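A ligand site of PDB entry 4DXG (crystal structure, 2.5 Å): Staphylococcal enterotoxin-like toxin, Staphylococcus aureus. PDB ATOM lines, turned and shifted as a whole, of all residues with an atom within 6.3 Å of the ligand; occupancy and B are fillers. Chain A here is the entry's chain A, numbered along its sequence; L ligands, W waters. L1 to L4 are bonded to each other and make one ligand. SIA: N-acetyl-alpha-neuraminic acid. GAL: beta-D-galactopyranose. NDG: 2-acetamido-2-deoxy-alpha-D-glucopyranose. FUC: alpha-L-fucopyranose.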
ATOM      1  N   LEU A 138       9.532 -20.989  17.561  1.00  0.00           N
ATOM      2  CA  LEU A 138       8.975 -20.230  18.660  1.00  0.00           C
ATOM      3  C   LEU A 138       8.295 -21.192  19.660  1.00  0.00           C
ATOM      4  O   LEU A 138       8.265 -20.908  20.842  1.00  0.00           O
ATOM      5  CB  LEU A 138       8.039 -19.148  18.172  1.00  0.00           C
ATOM      6  CG  LEU A 138       8.574 -18.219  17.102  1.00  0.00           C
ATOM      7  CD1 LEU A 138       7.421 -17.291  16.802  1.00  0.00           C
ATOM      8  CD2 LEU A 138       9.814 -17.410  17.540  1.00  0.00           C
ATOM      9  N   VAL A 165       9.408 -11.259  25.775  1.00  0.00           N
ATOM     10  CA  VAL A 165       9.964 -10.704  24.538  1.00  0.00           C
ATOM     11  C   VAL A 165      11.384 -11.190  24.218  1.00  0.00           C
ATOM     12  O   VAL A 165      12.341 -10.844  24.914  1.00  0.00           O
ATOM     13  CB  VAL A 165       9.930  -9.159  24.516  1.00  0.00           C
ATOM     14  CG1 VAL A 165      10.304  -8.645  23.138  1.00  0.00           C
ATOM     15  CG2 VAL A 165       8.514  -8.640  24.854  1.00  0.00           C
ATOM     16  N   MET A 168      16.360  -9.810  19.306  1.00  0.00           N
ATOM     17  CA  MET A 168      17.393 -10.267  18.355  1.00  0.00           C
ATOM     18  C   MET A 168      18.520  -9.249  18.079  1.00  0.00           C
ATOM     19  O   MET A 168      18.290  -8.049  18.075  1.00  0.00           O
ATOM     20  CB  MET A 168      16.783 -10.674  16.975  1.00  0.00           C
ATOM     21  CG  MET A 168      15.467 -11.459  16.976  1.00  0.00           C
ATOM     22  SD  MET A 168      15.615 -13.006  17.880  1.00  0.00           S
ATOM     23  CE  MET A 168      16.436 -14.064  16.644  1.00  0.00           C
ATOM     24  N   ASN A 170      19.583  -8.054  15.448  1.00  0.00           N
ATOM     25  CA  ASN A 170      19.177  -7.013  14.502  1.00  0.00           C
ATOM     26  C   ASN A 170      18.104  -6.010  15.000  1.00  0.00           C
ATOM     27  O   ASN A 170      17.666  -5.125  14.263  1.00  0.00           O
ATOM     28  CB  ASN A 170      18.732  -7.657  13.170  1.00  0.00           C
ATOM     29  CG  ASN A 170      17.392  -8.380  13.296  1.00  0.00           C
ATOM     30  OD1 ASN A 170      16.764  -8.398  14.370  1.00  0.00           O
ATOM     31  ND2 ASN A 170      16.942  -8.976  12.179  1.00  0.00           N
ATOM     32  N   GLY A 172      14.973  -6.962  15.801  1.00  0.00           N
ATOM     33  CA  GLY A 172      13.684  -7.632  15.727  1.00  0.00           C
ATOM     34  C   GLY A 172      13.329  -8.241  17.085  1.00  0.00           C
ATOM     35  O   GLY A 172      14.161  -8.264  18.012  1.00  0.00           O
ATOM     36  N   LYS A 173      12.091  -8.714  17.216  1.00  0.00           N
ATOM     37  CA  LYS A 173      11.575  -9.297  18.460  1.00  0.00           C
ATOM     38  C   LYS A 173      10.427 -10.275  18.211  1.00  0.00           C
ATOM     39  O   LYS A 173       9.810 -10.260  17.134  1.00  0.00           O
ATOM     40  CB  LYS A 173      11.100  -8.203  19.419  1.00  0.00           C
ATOM     41  CG  LYS A 173       9.836  -7.474  18.930  1.00  0.00           C
ATOM     42  CD  LYS A 173       9.348  -6.463  19.923  1.00  0.00           C
ATOM     43  CE  LYS A 173       8.355  -5.530  19.247  1.00  0.00           C
ATOM     44  NZ  LYS A 173       7.233  -5.268  20.211  1.00  0.00           N
ATOM     45  N   TYR A 174      10.143 -11.094  19.232  1.00  0.00           N
ATOM     46  CA  TYR A 174       9.074 -12.105  19.204  1.00  0.00           C
ATOM     47  C   TYR A 174       8.439 -12.163  20.560  1.00  0.00           C
ATOM     48  O   TYR A 174       9.120 -12.385  21.555  1.00  0.00           O
ATOM     49  CB  TYR A 174       9.634 -13.481  18.835  1.00  0.00           C
ATOM     50  CG  TYR A 174      10.330 -13.455  17.485  1.00  0.00           C
ATOM     51  CD1 TYR A 174      11.692 -13.200  17.399  1.00  0.00           C
ATOM     52  CD2 TYR A 174       9.620 -13.662  16.288  1.00  0.00           C
ATOM     53  CE1 TYR A 174      12.341 -13.152  16.178  1.00  0.00           C
ATOM     54  CE2 TYR A 174      10.257 -13.631  15.073  1.00  0.00           C
ATOM     55  CZ  TYR A 174      11.632 -13.379  15.007  1.00  0.00           C
ATOM     56  OH  TYR A 174      12.300 -13.353  13.794  1.00  0.00           O
ATOM     57  N   THR A 175       7.140 -11.928  20.611  1.00  0.00           N
ATOM     58  CA  THR A 175       6.432 -11.692  21.844  1.00  0.00           C
ATOM     59  C   THR A 175       5.497 -12.845  22.090  1.00  0.00           C
ATOM     60  O   THR A 175       4.737 -13.221  21.178  1.00  0.00           O
ATOM     61  CB  THR A 175       5.558 -10.367  21.734  1.00  0.00           C
ATOM     62  OG1 THR A 175       6.392  -9.258  21.415  1.00  0.00           O
ATOM     63  CG2 THR A 175       4.881 -10.055  23.054  1.00  0.00           C
ATOM     64  N   PHE A 176       5.539 -13.392  23.322  1.00  0.00           N
ATOM     65  CA  PHE A 176       4.541 -14.365  23.766  1.00  0.00           C
ATOM     66  C   PHE A 176       3.672 -13.771  24.877  1.00  0.00           C
ATOM     67  O   PHE A 176       4.164 -13.452  25.971  1.00  0.00           O
ATOM     68  CB  PHE A 176       5.203 -15.664  24.250  1.00  0.00           C
ATOM     69  CG  PHE A 176       6.316 -16.130  23.373  1.00  0.00           C
ATOM     70  CD1 PHE A 176       6.141 -16.218  21.992  1.00  0.00           C
ATOM     71  CD2 PHE A 176       7.526 -16.520  23.915  1.00  0.00           C
ATOM     72  CE1 PHE A 176       7.198 -16.655  21.150  1.00  0.00           C
ATOM     73  CE2 PHE A 176       8.596 -16.982  23.093  1.00  0.00           C
ATOM     74  CZ  PHE A 176       8.426 -17.044  21.698  1.00  0.00           C
ATOM     75  N   GLU A 177       2.396 -13.624  24.609  1.00  0.00           N
ATOM     76  CA  GLU A 177       1.499 -13.177  25.653  1.00  0.00           C
ATOM     77  C   GLU A 177       1.116 -14.333  26.574  1.00  0.00           C
ATOM     78  O   GLU A 177       0.685 -15.401  26.140  1.00  0.00           O
ATOM     79  CB  GLU A 177       0.273 -12.537  25.035  1.00  0.00           C
ATOM     80  CG  GLU A 177       0.576 -11.378  24.070  1.00  0.00           C
ATOM     81  CD  GLU A 177      -0.680 -10.975  23.305  1.00  0.00           C
ATOM     82  OE1 GLU A 177      -1.338  -9.999  23.775  1.00  0.00           O
ATOM     83  OE2 GLU A 177      -1.035 -11.643  22.280  1.00  0.00           O
ATOM     84  N   HIS A 179      -1.200 -14.707  29.034  1.00  0.00           N
ATOM     85  CA  HIS A 179      -2.581 -15.012  29.465  1.00  0.00           C
ATOM     86  C   HIS A 179      -3.327 -16.097  28.615  1.00  0.00           C
ATOM     87  O   HIS A 179      -4.410 -16.535  28.992  1.00  0.00           O
ATOM     88  CB  HIS A 179      -3.376 -13.735  29.549  1.00  0.00           C
ATOM     89  CG  HIS A 179      -3.598 -13.087  28.225  1.00  0.00           C
ATOM     90  ND1 HIS A 179      -2.651 -12.294  27.603  1.00  0.00           N
ATOM     91  CD2 HIS A 179      -4.662 -13.114  27.379  1.00  0.00           C
ATOM     92  CE1 HIS A 179      -3.127 -11.861  26.453  1.00  0.00           C
ATOM     93  NE2 HIS A 179      -4.345 -12.335  26.297  1.00  0.00           N
ATOM     94  N   LYS A 180      -2.718 -16.513  27.483  1.00  0.00           N
ATOM     95  CA  LYS A 180      -3.202 -17.612  26.616  1.00  0.00           C
ATOM     96  C   LYS A 180      -2.011 -18.376  25.965  1.00  0.00           C
ATOM     97  O   LYS A 180      -0.848 -17.865  25.979  1.00  0.00           O
ATOM     98  CB  LYS A 180      -4.092 -17.063  25.489  1.00  0.00           C
ATOM     99  CG  LYS A 180      -3.333 -16.126  24.534  1.00  0.00           C
ATOM    100  CD  LYS A 180      -4.251 -15.421  23.596  1.00  0.00           C
ATOM    101  CE  LYS A 180      -3.471 -14.364  22.846  1.00  0.00           C
ATOM    102  NZ  LYS A 180      -4.369 -13.599  21.939  1.00  0.00           N
ATOM    103  N   LEU A 182       0.341 -20.098  23.007  1.00  0.00           N
ATOM    104  CA  LEU A 182       0.965 -19.519  21.817  1.00  0.00           C
ATOM    105  C   LEU A 182      -0.022 -19.854  20.709  1.00  0.00           C
ATOM    106  O   LEU A 182      -0.622 -20.929  20.710  1.00  0.00           O
ATOM    107  CB  LEU A 182       2.342 -20.171  21.559  1.00  0.00           C
ATOM    108  CG  LEU A 182       3.047 -19.683  20.296  1.00  0.00           C
ATOM    109  CD1 LEU A 182       3.278 -18.164  20.363  1.00  0.00           C
ATOM    110  CD2 LEU A 182       4.379 -20.429  19.957  1.00  0.00           C
ATOM    111  N   GLN A 183      -0.256 -18.935  19.792  1.00  0.00           N
ATOM    112  CA  GLN A 183      -1.224 -19.262  18.748  1.00  0.00           C
ATOM    113  C   GLN A 183      -0.592 -20.334  17.883  1.00  0.00           C
ATOM    114  O   GLN A 183       0.579 -20.267  17.535  1.00  0.00           O
ATOM    115  CB  GLN A 183      -1.651 -18.023  17.944  1.00  0.00           C
ATOM    116  CG  GLN A 183      -2.055 -16.793  18.819  1.00  0.00           C
ATOM    117  CD  GLN A 183      -0.843 -15.904  19.160  1.00  0.00           C
ATOM    118  OE1 GLN A 183       0.249 -16.394  19.413  1.00  0.00           O
ATOM    119  NE2 GLN A 183      -1.053 -14.570  19.155  1.00  0.00           N
ATOM    120  N   GLU A 184      -1.383 -21.341  17.561  1.00  0.00           N
ATOM    121  CA  GLU A 184      -0.900 -22.529  16.874  1.00  0.00           C
ATOM    122  C   GLU A 184      -0.138 -22.298  15.606  1.00  0.00           C
ATOM    123  O   GLU A 184       0.825 -23.011  15.344  1.00  0.00           O
ATOM    124  CB  GLU A 184      -2.049 -23.501  16.657  1.00  0.00           C
ATOM    125  CG  GLU A 184      -2.053 -24.188  15.342  1.00  0.00           C
ATOM    126  CD  GLU A 184      -3.275 -25.055  15.205  1.00  0.00           C
ATOM    127  OE1 GLU A 184      -3.994 -24.892  14.172  1.00  0.00           O
ATOM    128  OE2 GLU A 184      -3.524 -25.854  16.190  1.00  0.00           O
ATOM    129  N   ASN A 185      -0.514 -21.291  14.841  1.00  0.00           N
ATOM    130  CA  ASN A 185       0.206 -21.003  13.596  1.00  0.00           C
ATOM    131  C   ASN A 185       1.682 -20.634  13.864  1.00  0.00           C
ATOM    132  O   ASN A 185       2.586 -20.927  13.061  1.00  0.00           O
ATOM    133  CB  ASN A 185      -0.556 -19.941  12.752  1.00  0.00           C
ATOM    134  CG  ASN A 185      -0.544 -18.532  13.363  1.00  0.00           C
ATOM    135  OD1 ASN A 185      -1.054 -18.294  14.458  1.00  0.00           O
ATOM    136  ND2 ASN A 185       0.015 -17.582  12.634  1.00  0.00           N
ATOM    137  N   ARG A 186       1.902 -20.028  15.026  1.00  0.00           N
ATOM    138  CA  ARG A 186       3.198 -19.505  15.403  1.00  0.00           C
ATOM    139  C   ARG A 186       4.125 -20.617  15.857  1.00  0.00           C
ATOM    140  O   ARG A 186       5.337 -20.472  15.834  1.00  0.00           O
ATOM    141  CB  ARG A 186       3.000 -18.457  16.505  1.00  0.00           C
ATOM    142  CG  ARG A 186       2.231 -17.228  16.025  1.00  0.00           C
ATOM    143  CD  ARG A 186       2.208 -16.160  17.056  1.00  0.00           C
ATOM    144  NE  ARG A 186       3.544 -15.571  17.296  1.00  0.00           N
ATOM    145  CZ  ARG A 186       3.898 -14.999  18.442  1.00  0.00           C
ATOM    146  NH1 ARG A 186       3.040 -14.948  19.475  1.00  0.00           N
ATOM    147  NH2 ARG A 186       5.097 -14.451  18.559  1.00  0.00           N
ATOM    148  N   ASP A 189       6.686 -21.152  13.325  1.00  0.00           N
ATOM    149  CA  ASP A 189       7.623 -20.079  13.018  1.00  0.00           C
ATOM    150  C   ASP A 189       9.021 -20.452  13.509  1.00  0.00           C
ATOM    151  O   ASP A 189       9.170 -21.019  14.595  1.00  0.00           O
ATOM    152  CB  ASP A 189       7.140 -18.744  13.614  1.00  0.00           C
ATOM    153  CG  ASP A 189       5.983 -18.094  12.806  1.00  0.00           C
ATOM    154  OD1 ASP A 189       5.898 -18.219  11.557  1.00  0.00           O
ATOM    155  OD2 ASP A 189       5.130 -17.431  13.437  1.00  0.00           O
HETATM  156  C1  SIA L   1       5.721  -9.792  17.907  1.00  0.00           C
HETATM  157  C2  SIA L   1       5.112  -9.405  16.540  1.00  0.00           C
HETATM  158  C3  SIA L   1       5.792  -8.102  16.057  1.00  0.00           C
HETATM  159  C4  SIA L   1       7.226  -8.321  15.576  1.00  0.00           C
HETATM  160  C5  SIA L   1       7.377  -9.508  14.605  1.00  0.00           C
HETATM  161  C6  SIA L   1       6.652 -10.714  15.209  1.00  0.00           C
HETATM  162  C7  SIA L   1       6.636 -11.966  14.314  1.00  0.00           C
HETATM  163  C8  SIA L   1       5.801 -13.059  14.956  1.00  0.00           C
HETATM  164  C9  SIA L   1       5.993 -14.426  14.284  1.00  0.00           C
HETATM  165  C10 SIA L   1       9.493  -9.717  13.310  1.00  0.00           C
HETATM  166  C11 SIA L   1      10.946 -10.028  13.449  1.00  0.00           C
HETATM  167  N5  SIA L   1       8.808  -9.778  14.452  1.00  0.00           N
HETATM  168  O1A SIA L   1       5.967  -8.866  18.731  1.00  0.00           O
HETATM  169  O1B SIA L   1       5.910 -11.015  18.169  1.00  0.00           O
HETATM  170  O4  SIA L   1       7.774  -7.166  14.902  1.00  0.00           O
HETATM  171  O6  SIA L   1       5.288 -10.360  15.496  1.00  0.00           O
HETATM  172  O7  SIA L   1       6.002 -11.627  13.104  1.00  0.00           O
HETATM  173  O8  SIA L   1       6.150 -13.085  16.360  1.00  0.00           O
HETATM  174  O9  SIA L   1       5.232 -15.417  15.012  1.00  0.00           O
HETATM  175  O10 SIA L   1       9.011  -9.464  12.209  1.00  0.00           O
HETATM  176  C1  GAL L   2       1.073 -11.716  16.528  1.00  0.00           C
HETATM  177  C2  GAL L   2       1.836 -10.449  16.197  1.00  0.00           C
HETATM  178  C3  GAL L   2       3.013 -10.281  17.109  1.00  0.00           C
HETATM  179  C4  GAL L   2       2.538 -10.272  18.581  1.00  0.00           C
HETATM  180  C5  GAL L   2       1.777 -11.574  18.849  1.00  0.00           C
HETATM  181  C6  GAL L   2       1.159 -11.479  20.214  1.00  0.00           C
HETATM  182  O2  GAL L   2       2.320 -10.568  14.908  1.00  0.00           O
HETATM  183  O3  GAL L   2       3.704  -9.116  16.715  1.00  0.00           O
HETATM  184  O4  GAL L   2       1.688  -9.147  18.875  1.00  0.00           O
HETATM  185  O5  GAL L   2       0.717 -11.745  17.908  1.00  0.00           O
HETATM  186  O6  GAL L   2       0.509 -12.701  20.498  1.00  0.00           O
HETATM  187  C1  NDG L   3      -2.091 -15.088  13.859  1.00  0.00           C
HETATM  188  C2  NDG L   3      -2.641 -14.536  15.176  1.00  0.00           C
HETATM  189  C3  NDG L   3      -2.037 -13.147  15.537  1.00  0.00           C
HETATM  190  C4  NDG L   3      -0.507 -13.098  15.432  1.00  0.00           C
HETATM  191  C5  NDG L   3      -0.079 -13.651  14.070  1.00  0.00           C
HETATM  192  C6  NDG L   3       1.449 -13.566  13.966  1.00  0.00           C
HETATM  193  C7  NDG L   3      -4.881 -15.316  15.954  1.00  0.00           C
HETATM  194  C8  NDG L   3      -6.380 -15.049  15.973  1.00  0.00           C
HETATM  195  O5  NDG L   3      -0.652 -14.940  13.795  1.00  0.00           O
HETATM  196  O3  NDG L   3      -2.278 -12.822  16.887  1.00  0.00           O
HETATM  197  O4  NDG L   3      -0.045 -11.742  15.600  1.00  0.00           O
HETATM  198  O6  NDG L   3       1.955 -14.467  13.010  1.00  0.00           O
HETATM  199  O7  NDG L   3      -4.450 -16.304  16.542  1.00  0.00           O
HETATM  200  N2  NDG L   3      -4.101 -14.457  15.265  1.00  0.00           N
HETATM  201  O1  NDG L   3      -2.666 -14.393  12.771  1.00  0.00           O
HETATM  202  C1  FUC L   4      -3.362 -11.918  17.096  1.00  0.00           C
HETATM  203  C2  FUC L   4      -3.797 -12.053  18.550  1.00  0.00           C
HETATM  204  C3  FUC L   4      -2.848 -11.396  19.493  1.00  0.00           C
HETATM  205  C4  FUC L   4      -2.667  -9.963  19.090  1.00  0.00           C
HETATM  206  C5  FUC L   4      -2.166  -9.923  17.633  1.00  0.00           C
HETATM  207  C6  FUC L   4      -1.935  -8.548  17.037  1.00  0.00           C
HETATM  208  O2  FUC L   4      -3.802 -13.399  18.964  1.00  0.00           O
HETATM  209  O3  FUC L   4      -3.479 -11.474  20.751  1.00  0.00           O
HETATM  210  O4  FUC L   4      -3.951  -9.370  19.356  1.00  0.00           O
HETATM  211  O5  FUC L   4      -3.092 -10.562  16.774  1.00  0.00           O
HETATM  212  O   HOH W   1       1.457 -14.664  22.044  1.00  0.00           O
HETATM  213  O   HOH W   2      -3.898  -9.892  23.464  1.00  0.00           O
HETATM  214  O   HOH W   3      10.233  -6.942  15.106  1.00  0.00           O
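An oxygen (O9) of SIA L1 sits at hydrogen-bond distance from the side-chain carboxylate (OD2) of Asp 189. OE2 of Glu 177 is in hydrogen-bond range of O6 of GAL L2 (2.6 Å). NZ of Lys 180 lies within hydrogen-bond range of O3 of FUC L4. O1B of SIA L1 sits at hydrogen-bond distance from N of Thr 175 (2.9 Å). O1A of SIA L1 is in hydrogen-bond range of OG1 of Thr 175 (2.7 Å). The side-chain amide nitrogen (NE2) of Gln 183 lies within hydrogen-bond range of an oxygen (O6) of GAL L2. An oxygen (O1B) of SIA L1 is in salt-bridge range of the guanidinium group (NH2) of Arg 186, at 3.6 Å. A nitrogen (N5) of SIA L1 lies within hydrogen-bond range of the backbone carbonyl oxygen of Lys 173 (2.9 Å). The side-chain amide nitrogen (ND2) of Asn 185 sits at hydrogen-bond distance from an oxygen (O5) of NDG L3 (3.0 Å).
The backbone NH of Leu 138 is in hydrogen-bond range of the backbone carbonyl oxygen of Asp 189 (3.0 Å). The side-chain carboxylate (OE2) of Glu 177 is in salt-bridge range of the side-chain amino group (NZ) of Lys 180 (3.9 Å). NH2 of Arg 186 is in hydrogen-bond range of O of Thr 175 (2.9 Å). The side-chain amide oxygen of Gln 183 lies close to the guanidinium group of Arg 186, at 3.1 Å.
CD1 of Leu 138 touches O9 of SIA L1, at 3.4 Å. CA of Tyr 174 touches O1B of SIA L1, at 3.5 Å. Hydrophobic or aromatic side chains that line the ligand: Leu 138 and Tyr 174. Ten residues have an atom within 4 Å of the ligand: Leu 138, Lys 173, Tyr 174, Thr 175, Glu 177, Lys 180, Gln 183, Asn 185, Arg 186 and Asp 189. The nearest printed residue that does not touch the ligand is Gly 172 (4.3 Å).
Water W3 bridges O4 of SIA L1 (2.5 Å) and N of Lys 173 (3.3 Å). Water W1 lies within hydrogen-bond range of an oxygen (O6) of GAL L2 (2.7 Å), the backbone NH (N) of Glu 177 (2.9 Å), the guanidinium group (NH1) of Arg 186 (3.0 Å) and the side-chain amide oxygen (OE1) of Gln 183 (3.4 Å). Water W2 bridges OE1 of Glu 177 and O3 of FUC L4.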
